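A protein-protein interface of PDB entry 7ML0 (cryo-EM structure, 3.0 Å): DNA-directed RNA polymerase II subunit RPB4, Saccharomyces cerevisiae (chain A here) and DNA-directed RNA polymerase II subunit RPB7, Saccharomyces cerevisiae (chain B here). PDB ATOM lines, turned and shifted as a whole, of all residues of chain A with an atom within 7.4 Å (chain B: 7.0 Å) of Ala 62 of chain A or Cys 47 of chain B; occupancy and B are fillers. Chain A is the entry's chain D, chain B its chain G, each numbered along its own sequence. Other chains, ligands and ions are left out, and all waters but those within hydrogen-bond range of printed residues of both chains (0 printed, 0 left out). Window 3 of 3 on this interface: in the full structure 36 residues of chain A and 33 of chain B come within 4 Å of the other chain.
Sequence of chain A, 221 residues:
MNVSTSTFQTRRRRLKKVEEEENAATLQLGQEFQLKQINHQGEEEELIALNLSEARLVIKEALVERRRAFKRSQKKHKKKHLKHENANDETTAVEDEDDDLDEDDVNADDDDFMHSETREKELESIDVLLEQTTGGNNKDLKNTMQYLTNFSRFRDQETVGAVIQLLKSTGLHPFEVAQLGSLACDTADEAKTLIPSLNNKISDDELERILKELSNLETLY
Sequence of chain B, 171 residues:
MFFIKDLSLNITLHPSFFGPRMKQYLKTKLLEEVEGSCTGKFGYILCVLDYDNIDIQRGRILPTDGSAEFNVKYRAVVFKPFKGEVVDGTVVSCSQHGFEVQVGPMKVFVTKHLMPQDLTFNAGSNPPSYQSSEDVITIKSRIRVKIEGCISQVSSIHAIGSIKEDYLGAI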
ATOM      1  N   ALA A  55     -11.007 -29.284  -3.423  1.00  0.00           N
ATOM      2  CA  ALA A  55     -10.239 -29.012  -4.625  1.00  0.00           C
ATOM      3  C   ALA A  55      -9.510 -27.690  -4.496  1.00  0.00           C
ATOM      4  O   ALA A  55      -8.344 -27.566  -4.887  1.00  0.00           O
ATOM      5  CB  ALA A  55     -11.162 -28.997  -5.834  1.00  0.00           C
ATOM      6  N   LEU A  57      -8.496 -26.807  -1.801  1.00  0.00           N
ATOM      7  CA  LEU A  57      -7.454 -27.120  -0.829  1.00  0.00           C
ATOM      8  C   LEU A  57      -6.277 -27.822  -1.478  1.00  0.00           C
ATOM      9  O   LEU A  57      -5.124 -27.425  -1.276  1.00  0.00           O
ATOM     10  CB  LEU A  57      -8.013 -27.972   0.307  1.00  0.00           C
ATOM     11  CG  LEU A  57      -7.959 -27.268   1.664  1.00  0.00           C
ATOM     12  CD1 LEU A  57      -8.356 -28.192   2.793  1.00  0.00           C
ATOM     13  CD2 LEU A  57      -6.580 -26.691   1.904  1.00  0.00           C
ATOM     14  N   VAL A  58      -6.539 -28.867  -2.259  1.00  0.00           N
ATOM     15  CA  VAL A  58      -5.436 -29.622  -2.847  1.00  0.00           C
ATOM     16  C   VAL A  58      -4.591 -28.719  -3.729  1.00  0.00           C
ATOM     17  O   VAL A  58      -3.359 -28.803  -3.725  1.00  0.00           O
ATOM     18  CB  VAL A  58      -5.973 -30.840  -3.615  1.00  0.00           C
ATOM     19  CG1 VAL A  58      -6.884 -30.396  -4.726  1.00  0.00           C
ATOM     20  CG2 VAL A  58      -4.835 -31.677  -4.145  1.00  0.00           C
ATOM     21  N   ILE A  59      -5.238 -27.826  -4.475  1.00  0.00           N
ATOM     22  CA  ILE A  59      -4.521 -26.834  -5.266  1.00  0.00           C
ATOM     23  C   ILE A  59      -3.487 -26.127  -4.405  1.00  0.00           C
ATOM     24  O   ILE A  59      -2.283 -26.203  -4.663  1.00  0.00           O
ATOM     25  CB  ILE A  59      -5.512 -25.834  -5.887  1.00  0.00           C
ATOM     26  CG1 ILE A  59      -6.070 -26.395  -7.186  1.00  0.00           C
ATOM     27  CG2 ILE A  59      -4.859 -24.512  -6.149  1.00  0.00           C
ATOM     28  CD1 ILE A  59      -6.733 -25.363  -8.061  1.00  0.00           C
ATOM     29  N   LYS A  60      -3.948 -25.483  -3.328  1.00  0.00           N
ATOM     30  CA  LYS A  60      -3.046 -24.741  -2.454  1.00  0.00           C
ATOM     31  C   LYS A  60      -1.915 -25.622  -1.968  1.00  0.00           C
ATOM     32  O   LYS A  60      -0.755 -25.200  -1.947  1.00  0.00           O
ATOM     33  CB  LYS A  60      -3.813 -24.179  -1.260  1.00  0.00           C
ATOM     34  CG  LYS A  60      -2.942 -23.930  -0.038  1.00  0.00           C
ATOM     35  CD  LYS A  60      -3.756 -23.927   1.243  1.00  0.00           C
ATOM     36  CE  LYS A  60      -2.868 -23.752   2.457  1.00  0.00           C
ATOM     37  NZ  LYS A  60      -3.624 -23.910   3.728  1.00  0.00           N
ATOM     38  N   GLU A  61      -2.239 -26.851  -1.578  1.00  0.00           N
ATOM     39  CA  GLU A  61      -1.205 -27.805  -1.216  1.00  0.00           C
ATOM     40  C   GLU A  61      -0.171 -27.918  -2.320  1.00  0.00           C
ATOM     41  O   GLU A  61       1.034 -27.792  -2.080  1.00  0.00           O
ATOM     42  CB  GLU A  61      -1.831 -29.160  -0.946  1.00  0.00           C
ATOM     43  CG  GLU A  61      -0.849 -30.277  -1.040  1.00  0.00           C
ATOM     44  CD  GLU A  61      -1.529 -31.600  -0.935  1.00  0.00           C
ATOM     45  OE1 GLU A  61      -2.774 -31.619  -0.978  1.00  0.00           O
ATOM     46  OE2 GLU A  61      -0.822 -32.617  -0.816  1.00  0.00           O
ATOM     47  N   ALA A  62      -0.634 -28.126  -3.545  1.00  0.00           N
ATOM     48  CA  ALA A  62       0.281 -28.226  -4.667  1.00  0.00           C
ATOM     49  C   ALA A  62       1.050 -26.930  -4.865  1.00  0.00           C
ATOM     50  O   ALA A  62       2.282 -26.932  -4.896  1.00  0.00           O
ATOM     51  CB  ALA A  62      -0.500 -28.594  -5.923  1.00  0.00           C
ATOM     52  N   LEU A  63       0.342 -25.807  -4.966  1.00  0.00           N
ATOM     53  CA  LEU A  63       1.025 -24.550  -5.243  1.00  0.00           C
ATOM     54  C   LEU A  63       2.071 -24.270  -4.183  1.00  0.00           C
ATOM     55  O   LEU A  63       3.185 -23.830  -4.492  1.00  0.00           O
ATOM     56  CB  LEU A  63       0.034 -23.393  -5.299  1.00  0.00           C
ATOM     57  CG  LEU A  63      -1.387 -23.570  -5.827  1.00  0.00           C
ATOM     58  CD1 LEU A  63      -2.033 -22.220  -6.070  1.00  0.00           C
ATOM     59  CD2 LEU A  63      -1.408 -24.397  -7.083  1.00  0.00           C
ATOM     60  N   VAL A  64       1.729 -24.524  -2.925  1.00  0.00           N
ATOM     61  CA  VAL A  64       2.710 -24.401  -1.859  1.00  0.00           C
ATOM     62  C   VAL A  64       3.790 -25.458  -2.012  1.00  0.00           C
ATOM     63  O   VAL A  64       4.985 -25.152  -2.006  1.00  0.00           O
ATOM     64  CB  VAL A  64       2.022 -24.504  -0.492  1.00  0.00           C
ATOM     65  CG1 VAL A  64       3.030 -24.890   0.558  1.00  0.00           C
ATOM     66  CG2 VAL A  64       1.360 -23.192  -0.147  1.00  0.00           C
ATOM     67  N   GLU A  65       3.387 -26.714  -2.179  1.00  0.00           N
ATOM     68  CA  GLU A  65       4.379 -27.769  -2.323  1.00  0.00           C
ATOM     69  C   GLU A  65       5.338 -27.445  -3.451  1.00  0.00           C
ATOM     70  O   GLU A  65       6.505 -27.848  -3.420  1.00  0.00           O
ATOM     71  CB  GLU A  65       3.684 -29.107  -2.559  1.00  0.00           C
ATOM     72  CG  GLU A  65       4.395 -30.045  -3.488  1.00  0.00           C
ATOM     73  CD  GLU A  65       5.642 -30.630  -2.883  1.00  0.00           C
ATOM     74  OE1 GLU A  65       6.173 -30.056  -1.910  1.00  0.00           O
ATOM     75  OE2 GLU A  65       6.098 -31.676  -3.380  1.00  0.00           O
ATOM     76  N   ARG A  66       4.866 -26.695  -4.439  1.00  0.00           N
ATOM     77  CA  ARG A  66       5.763 -26.077  -5.395  1.00  0.00           C
ATOM     78  C   ARG A  66       6.442 -24.858  -4.805  1.00  0.00           C
ATOM     79  O   ARG A  66       7.602 -24.586  -5.124  1.00  0.00           O
ATOM     80  CB  ARG A  66       4.995 -25.682  -6.646  1.00  0.00           C
ATOM     81  CG  ARG A  66       5.836 -25.638  -7.885  1.00  0.00           C
ATOM     82  CD  ARG A  66       4.979 -25.294  -9.076  1.00  0.00           C
ATOM     83  NE  ARG A  66       3.831 -26.184  -9.190  1.00  0.00           N
ATOM     84  CZ  ARG A  66       2.720 -25.873  -9.845  1.00  0.00           C
ATOM     85  NH1 ARG A  66       2.611 -24.696 -10.437  1.00  0.00           N
ATOM     86  NH2 ARG A  66       1.723 -26.736  -9.906  1.00  0.00           N
ATOM     87  N   ARG A  67       5.746 -24.112  -3.951  1.00  0.00           N
ATOM     88  CA  ARG A  67       6.346 -22.897  -3.417  1.00  0.00           C
ATOM     89  C   ARG A  67       7.532 -23.226  -2.532  1.00  0.00           C
ATOM     90  O   ARG A  67       8.518 -22.488  -2.505  1.00  0.00           O
ATOM     91  CB  ARG A  67       5.315 -22.077  -2.652  1.00  0.00           C
ATOM     92  CG  ARG A  67       5.492 -20.594  -2.853  1.00  0.00           C
ATOM     93  CD  ARG A  67       4.959 -19.797  -1.677  1.00  0.00           C
ATOM     94  NE  ARG A  67       5.697 -20.038  -0.434  1.00  0.00           N
ATOM     95  CZ  ARG A  67       5.321 -20.894   0.513  1.00  0.00           C
ATOM     96  NH1 ARG A  67       4.214 -21.605   0.367  1.00  0.00           N
ATOM     97  NH2 ARG A  67       6.052 -21.039   1.606  1.00  0.00           N
ATOM     98  N   ARG A  68       7.459 -24.328  -1.793  1.00  0.00           N
ATOM     99  CA  ARG A  68       8.677 -24.824  -1.174  1.00  0.00           C
ATOM    100  C   ARG A  68       9.632 -25.368  -2.223  1.00  0.00           C
ATOM    101  O   ARG A  68      10.849 -25.223  -2.085  1.00  0.00           O
ATOM    102  CB  ARG A  68       8.353 -25.890  -0.131  1.00  0.00           C
ATOM    103  CG  ARG A  68       7.787 -27.156  -0.701  1.00  0.00           C
ATOM    104  CD  ARG A  68       7.938 -28.324   0.254  1.00  0.00           C
ATOM    105  NE  ARG A  68       6.800 -28.469   1.158  1.00  0.00           N
ATOM    106  CZ  ARG A  68       6.829 -28.181   2.455  1.00  0.00           C
ATOM    107  NH1 ARG A  68       7.942 -27.731   3.017  1.00  0.00           N
ATOM    108  NH2 ARG A  68       5.744 -28.349   3.193  1.00  0.00           N
ATOM    109  N   ALA A  69       9.099 -25.961  -3.295  1.00  0.00           N
ATOM    110  CA  ALA A  69       9.937 -26.654  -4.267  1.00  0.00           C
ATOM    111  C   ALA A  69      10.517 -25.697  -5.298  1.00  0.00           C
ATOM    112  O   ALA A  69      11.731 -25.686  -5.524  1.00  0.00           O
ATOM    113  CB  ALA A  69       9.139 -27.756  -4.958  1.00  0.00           C
ATOM    114  N   LEU A 130       1.602 -17.166  -4.134  1.00  0.00           N
ATOM    115  CA  LEU A 130       1.785 -18.334  -4.975  1.00  0.00           C
ATOM    116  C   LEU A 130       1.743 -17.982  -6.453  1.00  0.00           C
ATOM    117  O   LEU A 130       2.269 -18.738  -7.273  1.00  0.00           O
ATOM    118  CB  LEU A 130       0.715 -19.371  -4.649  1.00  0.00           C
ATOM    119  CG  LEU A 130       0.735 -19.868  -3.206  1.00  0.00           C
ATOM    120  CD1 LEU A 130      -0.596 -20.493  -2.855  1.00  0.00           C
ATOM    121  CD2 LEU A 130       1.847 -20.872  -3.023  1.00  0.00           C
ATOM    122  N   THR A 133       5.093 -17.598  -7.890  1.00  0.00           N
ATOM    123  CA  THR A 133       5.643 -18.943  -7.984  1.00  0.00           C
ATOM    124  C   THR A 133       5.169 -19.654  -9.248  1.00  0.00           C
ATOM    125  O   THR A 133       5.886 -20.505  -9.784  1.00  0.00           O
ATOM    126  CB  THR A 133       5.261 -19.729  -6.730  1.00  0.00           C
ATOM    127  OG1 THR A 133       5.387 -18.879  -5.583  1.00  0.00           O
ATOM    128  CG2 THR A 133       6.164 -20.923  -6.547  1.00  0.00           C
ATOM    129  N   ASN A 138      -2.350 -16.647 -14.660  1.00  0.00           N
ATOM    130  CA  ASN A 138      -3.254 -17.600 -14.049  1.00  0.00           C
ATOM    131  C   ASN A 138      -4.165 -16.961 -13.015  1.00  0.00           C
ATOM    132  O   ASN A 138      -4.789 -17.650 -12.215  1.00  0.00           O
ATOM    133  CB  ASN A 138      -2.454 -18.742 -13.438  1.00  0.00           C
ATOM    134  CG  ASN A 138      -2.188 -19.846 -14.425  1.00  0.00           C
ATOM    135  OD1 ASN A 138      -2.540 -19.740 -15.596  1.00  0.00           O
ATOM    136  ND2 ASN A 138      -1.561 -20.912 -13.965  1.00  0.00           N
ATOM    137  N   LEU A 141      -6.622 -18.844 -13.613  1.00  0.00           N
ATOM    138  CA  LEU A 141      -6.658 -19.938 -12.647  1.00  0.00           C
ATOM    139  C   LEU A 141      -7.154 -19.424 -11.305  1.00  0.00           C
ATOM    140  O   LEU A 141      -7.914 -20.108 -10.610  1.00  0.00           O
ATOM    141  CB  LEU A 141      -5.282 -20.591 -12.498  1.00  0.00           C
ATOM    142  CG  LEU A 141      -4.764 -20.807 -11.061  1.00  0.00           C
ATOM    143  CD1 LEU A 141      -5.367 -22.026 -10.396  1.00  0.00           C
ATOM    144  CD2 LEU A 141      -3.271 -20.914 -11.012  1.00  0.00           C
ATOM    145  N   ILE B   4      -9.389 -34.636 -10.957  1.00  0.00           N
ATOM    146  CA  ILE B   4      -7.960 -34.827 -11.112  1.00  0.00           C
ATOM    147  C   ILE B   4      -7.761 -36.006 -12.039  1.00  0.00           C
ATOM    148  O   ILE B   4      -8.476 -37.010 -11.953  1.00  0.00           O
ATOM    149  CB  ILE B   4      -7.245 -35.041  -9.775  1.00  0.00           C
ATOM    150  CG1 ILE B   4      -6.213 -33.942  -9.609  1.00  0.00           C
ATOM    151  CG2 ILE B   4      -6.565 -36.386  -9.731  1.00  0.00           C
ATOM    152  CD1 ILE B   4      -5.858 -33.682  -8.190  1.00  0.00           C
ATOM    153  N   LEU B  31       4.622 -26.671 -17.330  1.00  0.00           N
ATOM    154  CA  LEU B  31       3.771 -25.780 -16.563  1.00  0.00           C
ATOM    155  C   LEU B  31       3.471 -24.524 -17.354  1.00  0.00           C
ATOM    156  O   LEU B  31       2.309 -24.143 -17.516  1.00  0.00           O
ATOM    157  CB  LEU B  31       4.435 -25.427 -15.243  1.00  0.00           C
ATOM    158  CG  LEU B  31       5.274 -26.522 -14.604  1.00  0.00           C
ATOM    159  CD1 LEU B  31       6.134 -25.960 -13.488  1.00  0.00           C
ATOM    160  CD2 LEU B  31       4.389 -27.610 -14.075  1.00  0.00           C
ATOM    161  N   VAL B  34       1.053 -25.706 -20.262  1.00  0.00           N
ATOM    162  CA  VAL B  34      -0.091 -26.571 -20.067  1.00  0.00           C
ATOM    163  C   VAL B  34      -1.054 -26.010 -19.032  1.00  0.00           C
ATOM    164  O   VAL B  34      -2.272 -26.124 -19.192  1.00  0.00           O
ATOM    165  CB  VAL B  34       0.345 -27.999 -19.704  1.00  0.00           C
ATOM    166  CG1 VAL B  34       0.364 -28.214 -18.215  1.00  0.00           C
ATOM    167  CG2 VAL B  34      -0.563 -28.975 -20.367  1.00  0.00           C
ATOM    168  N   GLU B  35      -0.542 -25.374 -17.985  1.00  0.00           N
ATOM    169  CA  GLU B  35      -1.414 -24.769 -16.994  1.00  0.00           C
ATOM    170  C   GLU B  35      -2.296 -23.718 -17.644  1.00  0.00           C
ATOM    171  O   GLU B  35      -1.879 -23.024 -18.570  1.00  0.00           O
ATOM    172  CB  GLU B  35      -0.589 -24.131 -15.890  1.00  0.00           C
ATOM    173  CG  GLU B  35      -0.511 -24.945 -14.628  1.00  0.00           C
ATOM    174  CD  GLU B  35       0.434 -24.333 -13.614  1.00  0.00           C
ATOM    175  OE1 GLU B  35       1.030 -23.287 -13.925  1.00  0.00           O
ATOM    176  OE2 GLU B  35       0.589 -24.896 -12.513  1.00  0.00           O
ATOM    177  N   GLY B  36      -3.526 -23.614 -17.166  1.00  0.00           N
ATOM    178  CA  GLY B  36      -4.388 -22.553 -17.637  1.00  0.00           C
ATOM    179  C   GLY B  36      -4.708 -22.613 -19.111  1.00  0.00           C
ATOM    180  O   GLY B  36      -4.822 -21.570 -19.757  1.00  0.00           O
ATOM    181  N   TYR B  44     -10.101 -27.153 -18.780  1.00  0.00           N
ATOM    182  CA  TYR B  44      -9.056 -26.239 -18.364  1.00  0.00           C
ATOM    183  C   TYR B  44      -8.072 -26.966 -17.478  1.00  0.00           C
ATOM    184  O   TYR B  44      -8.415 -27.380 -16.375  1.00  0.00           O
ATOM    185  CB  TYR B  44      -9.664 -25.064 -17.623  1.00  0.00           C
ATOM    186  CG  TYR B  44     -10.612 -24.300 -18.477  1.00  0.00           C
ATOM    187  CD1 TYR B  44     -11.923 -24.696 -18.608  1.00  0.00           C
ATOM    188  CD2 TYR B  44     -10.191 -23.193 -19.171  1.00  0.00           C
ATOM    189  CE1 TYR B  44     -12.793 -24.002 -19.401  1.00  0.00           C
ATOM    190  CE2 TYR B  44     -11.052 -22.488 -19.963  1.00  0.00           C
ATOM    191  CZ  TYR B  44     -12.352 -22.896 -20.077  1.00  0.00           C
ATOM    192  OH  TYR B  44     -13.206 -22.189 -20.877  1.00  0.00           O
ATOM    193  N   ILE B  45      -6.852 -27.132 -17.950  1.00  0.00           N
ATOM    194  CA  ILE B  45      -5.814 -27.720 -17.122  1.00  0.00           C
ATOM    195  C   ILE B  45      -5.412 -26.667 -16.113  1.00  0.00           C
ATOM    196  O   ILE B  45      -4.929 -25.593 -16.485  1.00  0.00           O
ATOM    197  CB  ILE B  45      -4.608 -28.170 -17.948  1.00  0.00           C
ATOM    198  CG1 ILE B  45      -4.938 -29.429 -18.729  1.00  0.00           C
ATOM    199  CG2 ILE B  45      -3.441 -28.439 -17.035  1.00  0.00           C
ATOM    200  CD1 ILE B  45      -5.645 -29.170 -20.002  1.00  0.00           C
ATOM    201  N   LEU B  46      -5.630 -26.955 -14.838  1.00  0.00           N
ATOM    202  CA  LEU B  46      -5.460 -25.939 -13.820  1.00  0.00           C
ATOM    203  C   LEU B  46      -4.152 -26.091 -13.068  1.00  0.00           C
ATOM    204  O   LEU B  46      -3.312 -25.190 -13.076  1.00  0.00           O
ATOM    205  CB  LEU B  46      -6.639 -26.001 -12.860  1.00  0.00           C
ATOM    206  CG  LEU B  46      -7.945 -25.976 -13.636  1.00  0.00           C
ATOM    207  CD1 LEU B  46      -9.108 -26.216 -12.723  1.00  0.00           C
ATOM    208  CD2 LEU B  46      -8.085 -24.651 -14.348  1.00  0.00           C
ATOM    209  N   CYS B  47      -3.957 -27.228 -12.422  1.00  0.00           N
ATOM    210  CA  CYS B  47      -2.806 -27.407 -11.560  1.00  0.00           C
ATOM    211  C   CYS B  47      -2.048 -28.628 -12.006  1.00  0.00           C
ATOM    212  O   CYS B  47      -2.573 -29.740 -11.946  1.00  0.00           O
ATOM    213  CB  CYS B  47      -3.212 -27.575 -10.102  1.00  0.00           C
ATOM    214  SG  CYS B  47      -1.913 -28.349  -9.120  1.00  0.00           S
ATOM    215  N   VAL B  48      -0.809 -28.433 -12.408  1.00  0.00           N
ATOM    216  CA  VAL B  48       0.078 -29.557 -12.631  1.00  0.00           C
ATOM    217  C   VAL B  48       0.599 -29.965 -11.266  1.00  0.00           C
ATOM    218  O   VAL B  48       1.460 -29.298 -10.690  1.00  0.00           O
ATOM    219  CB  VAL B  48       1.218 -29.200 -13.581  1.00  0.00           C
ATOM    220  CG1 VAL B  48       1.756 -30.449 -14.207  1.00  0.00           C
ATOM    221  CG2 VAL B  48       0.734 -28.237 -14.631  1.00  0.00           C
ATOM    222  N   LEU B  49       0.058 -31.037 -10.729  1.00  0.00           N
ATOM    223  CA  LEU B  49       0.535 -31.533  -9.458  1.00  0.00           C
ATOM    224  C   LEU B  49       1.501 -32.672  -9.695  1.00  0.00           C
ATOM    225  O   LEU B  49       1.745 -33.083 -10.828  1.00  0.00           O
ATOM    226  CB  LEU B  49      -0.622 -32.000  -8.603  1.00  0.00           C
ATOM    227  CG  LEU B  49      -1.360 -33.086  -9.348  1.00  0.00           C
ATOM    228  CD1 LEU B  49      -1.259 -34.412  -8.600  1.00  0.00           C
ATOM    229  CD2 LEU B  49      -2.779 -32.629  -9.525  1.00  0.00           C
ATOM    230  N   ASP B  50       2.035 -33.196  -8.601  1.00  0.00           N
ATOM    231  CA  ASP B  50       3.054 -34.230  -8.665  1.00  0.00           C
ATOM    232  C   ASP B  50       4.259 -33.745  -9.463  1.00  0.00           C
ATOM    233  O   ASP B  50       4.900 -34.508 -10.184  1.00  0.00           O
ATOM    234  CB  ASP B  50       2.482 -35.516  -9.255  1.00  0.00           C
ATOM    235  CG  ASP B  50       3.283 -36.732  -8.886  1.00  0.00           C
ATOM    236  OD1 ASP B  50       4.521 -36.644  -8.790  1.00  0.00           O
ATOM    237  OD2 ASP B  50       2.662 -37.793  -8.692  1.00  0.00           O
ATOM    238  N   TYR B  51       4.603 -32.468  -9.284  1.00  0.00           N
ATOM    239  CA  TYR B  51       5.680 -31.840 -10.044  1.00  0.00           C
ATOM    240  C   TYR B  51       7.001 -32.578  -9.913  1.00  0.00           C
ATOM    241  O   TYR B  51       7.965 -32.234 -10.601  1.00  0.00           O
ATOM    242  CB  TYR B  51       5.840 -30.389  -9.604  1.00  0.00           C
ATOM    243  CG  TYR B  51       6.982 -29.677 -10.260  1.00  0.00           C
ATOM    244  CD1 TYR B  51       6.946 -29.366 -11.598  1.00  0.00           C
ATOM    245  CD2 TYR B  51       8.109 -29.327  -9.539  1.00  0.00           C
ATOM    246  CE1 TYR B  51       7.996 -28.716 -12.201  1.00  0.00           C
ATOM    247  CE2 TYR B  51       9.163 -28.681 -10.133  1.00  0.00           C
ATOM    248  CZ  TYR B  51       9.100 -28.379 -11.468  1.00  0.00           C
ATOM    249  OH  TYR B  51      10.149 -27.730 -12.073  1.00  0.00           O
ATOM    250  N   TYR B  74       1.508 -37.141 -16.948  1.00  0.00           N
ATOM    251  CA  TYR B  74       1.454 -36.398 -15.700  1.00  0.00           C
ATOM    252  C   TYR B  74       0.033 -36.412 -15.157  1.00  0.00           C
ATOM    253  O   TYR B  74      -0.880 -36.971 -15.768  1.00  0.00           O
ATOM    254  CB  TYR B  74       1.955 -34.969 -15.898  1.00  0.00           C
ATOM    255  CG  TYR B  74       1.094 -34.113 -16.782  1.00  0.00           C
ATOM    256  CD1 TYR B  74       0.241 -34.662 -17.699  1.00  0.00           C
ATOM    257  CD2 TYR B  74       1.146 -32.747 -16.702  1.00  0.00           C
ATOM    258  CE1 TYR B  74      -0.524 -33.888 -18.494  1.00  0.00           C
ATOM    259  CE2 TYR B  74       0.375 -31.967 -17.505  1.00  0.00           C
ATOM    260  CZ  TYR B  74      -0.460 -32.545 -18.394  1.00  0.00           C
ATOM    261  OH  TYR B  74      -1.231 -31.772 -19.200  1.00  0.00           O
ATOM    262  N   ARG B  75      -0.149 -35.773 -13.998  1.00  0.00           N
ATOM    263  CA  ARG B  75      -1.434 -35.692 -13.317  1.00  0.00           C
ATOM    264  C   ARG B  75      -1.775 -34.242 -13.023  1.00  0.00           C
ATOM    265  O   ARG B  75      -0.906 -33.463 -12.628  1.00  0.00           O
ATOM    266  CB  ARG B  75      -1.431 -36.471 -12.023  1.00  0.00           C
ATOM    267  CG  ARG B  75      -2.766 -36.440 -11.313  1.00  0.00           C
ATOM    268  CD  ARG B  75      -2.994 -37.653 -10.422  1.00  0.00           C
ATOM    269  NE  ARG B  75      -1.898 -37.835  -9.486  1.00  0.00           N
ATOM    270  CZ  ARG B  75      -0.885 -38.672  -9.680  1.00  0.00           C
ATOM    271  NH1 ARG B  75      -0.842 -39.410 -10.781  1.00  0.00           N
ATOM    272  NH2 ARG B  75       0.084 -38.760  -8.778  1.00  0.00           N
ATOM    273  N   ALA B  76      -3.038 -33.887 -13.206  1.00  0.00           N
ATOM    274  CA  ALA B  76      -3.441 -32.502 -13.049  1.00  0.00           C
ATOM    275  C   ALA B  76      -4.938 -32.430 -12.798  1.00  0.00           C
ATOM    276  O   ALA B  76      -5.646 -33.439 -12.817  1.00  0.00           O
ATOM    277  CB  ALA B  76      -3.054 -31.682 -14.275  1.00  0.00           C
ATOM    278  N   VAL B  77      -5.420 -31.214 -12.579  1.00  0.00           N
ATOM    279  CA  VAL B  77      -6.803 -30.973 -12.206  1.00  0.00           C
ATOM    280  C   VAL B  77      -7.451 -30.104 -13.271  1.00  0.00           C
ATOM    281  O   VAL B  77      -6.797 -29.248 -13.875  1.00  0.00           O
ATOM    282  CB  VAL B  77      -6.893 -30.316 -10.818  1.00  0.00           C
ATOM    283  CG1 VAL B  77      -5.614 -30.542 -10.080  1.00  0.00           C
ATOM    284  CG2 VAL B  77      -7.146 -28.847 -10.938  1.00  0.00           C
ATOM    285  N   VAL B  78      -8.730 -30.336 -13.512  1.00  0.00           N
ATOM    286  CA  VAL B  78      -9.395 -29.738 -14.654  1.00  0.00           C
ATOM    287  C   VAL B  78     -10.834 -29.431 -14.321  1.00  0.00           C
ATOM    288  O   VAL B  78     -11.557 -30.275 -13.783  1.00  0.00           O
ATOM    289  CB  VAL B  78      -9.347 -30.659 -15.868  1.00  0.00           C
ATOM    290  CG1 VAL B  78      -8.068 -30.457 -16.604  1.00  0.00           C
ATOM    291  CG2 VAL B  78      -9.463 -32.066 -15.395  1.00  0.00           C
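The guanidinium group (NH2) of Arg 66 of chain A lies within hydrogen-bond range of the backbone carbonyl oxygen (O) of Val 48 of chain B, at 2.7 Å. The guanidinium group (NH1) of Arg 66 of chain A lies within salt-bridge range of the side-chain carboxylate (OE2) of Glu 35 of chain B (2.9 Å).
N of Leu 49 of chain B lies close to SG of Cys 47 of chain B, 3.7 Å away. The backbone NH (N) of Val 77 of chain B lies within hydrogen-bond range of the backbone carbonyl oxygen (O) of Cys 47 of chain B, at 3.3 Å. The backbone carbonyl oxygen (O) of Ile 45 of chain B sits at hydrogen-bond distance from the backbone NH (N) of Gly 36 of chain B, at 2.5 Å.
Cys 47 of chain B touches Ala 62 of chain A (SG to CB, 3.5 Å). ND2 of Asn 138 of chain A touches OE1 of Glu 35 of chain B (3.5 Å). Asn 138 of chain A touches Gly 36 of chain B.
Ala 62 of chain A touches one residue of chain B. Of the printed residues of chain B, Arg 66 of chain A touches Glu 35 (2.9 Å) and Val 48 (2.7 Å). Of the printed residues of chain B, Asn 138 of chain A touches Glu 35 and Gly 36. Of the printed residues of chain A, Glu 35 of chain B touches Arg 66 and Asn 138. Of the printed residues of chain A, Gly 36 of chain B touches Asn 138 (3.9 Å). Of chain A, only Ala 62 comes within 4 Å of Cys 47 of chain B. Arg 75 of chain B touches none of the printed residues of chain A. The nearest residue of chain A that does not touch Cys 47 of chain B is Arg 66 of chain A (4.1 Å). The nearest printed residue of chain A that does not touch Val 48 of chain B is Ala 62 of chain A (5.2 Å).
Printed residues of chain A that touch a printed residue of chain B: Ala 62, Arg 66 and Asn 138. Printed residues of chain B that touch a printed residue of chain A: Glu 35, Gly 36, Cys 47 and Val 48. Among the printed residues, Asp or Glu carboxylates within 4 Å of a Lys or Arg side-chain nitrogen of the other chain: Arg 66 of chain A with Glu 35 of chain B (2.9 Å).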
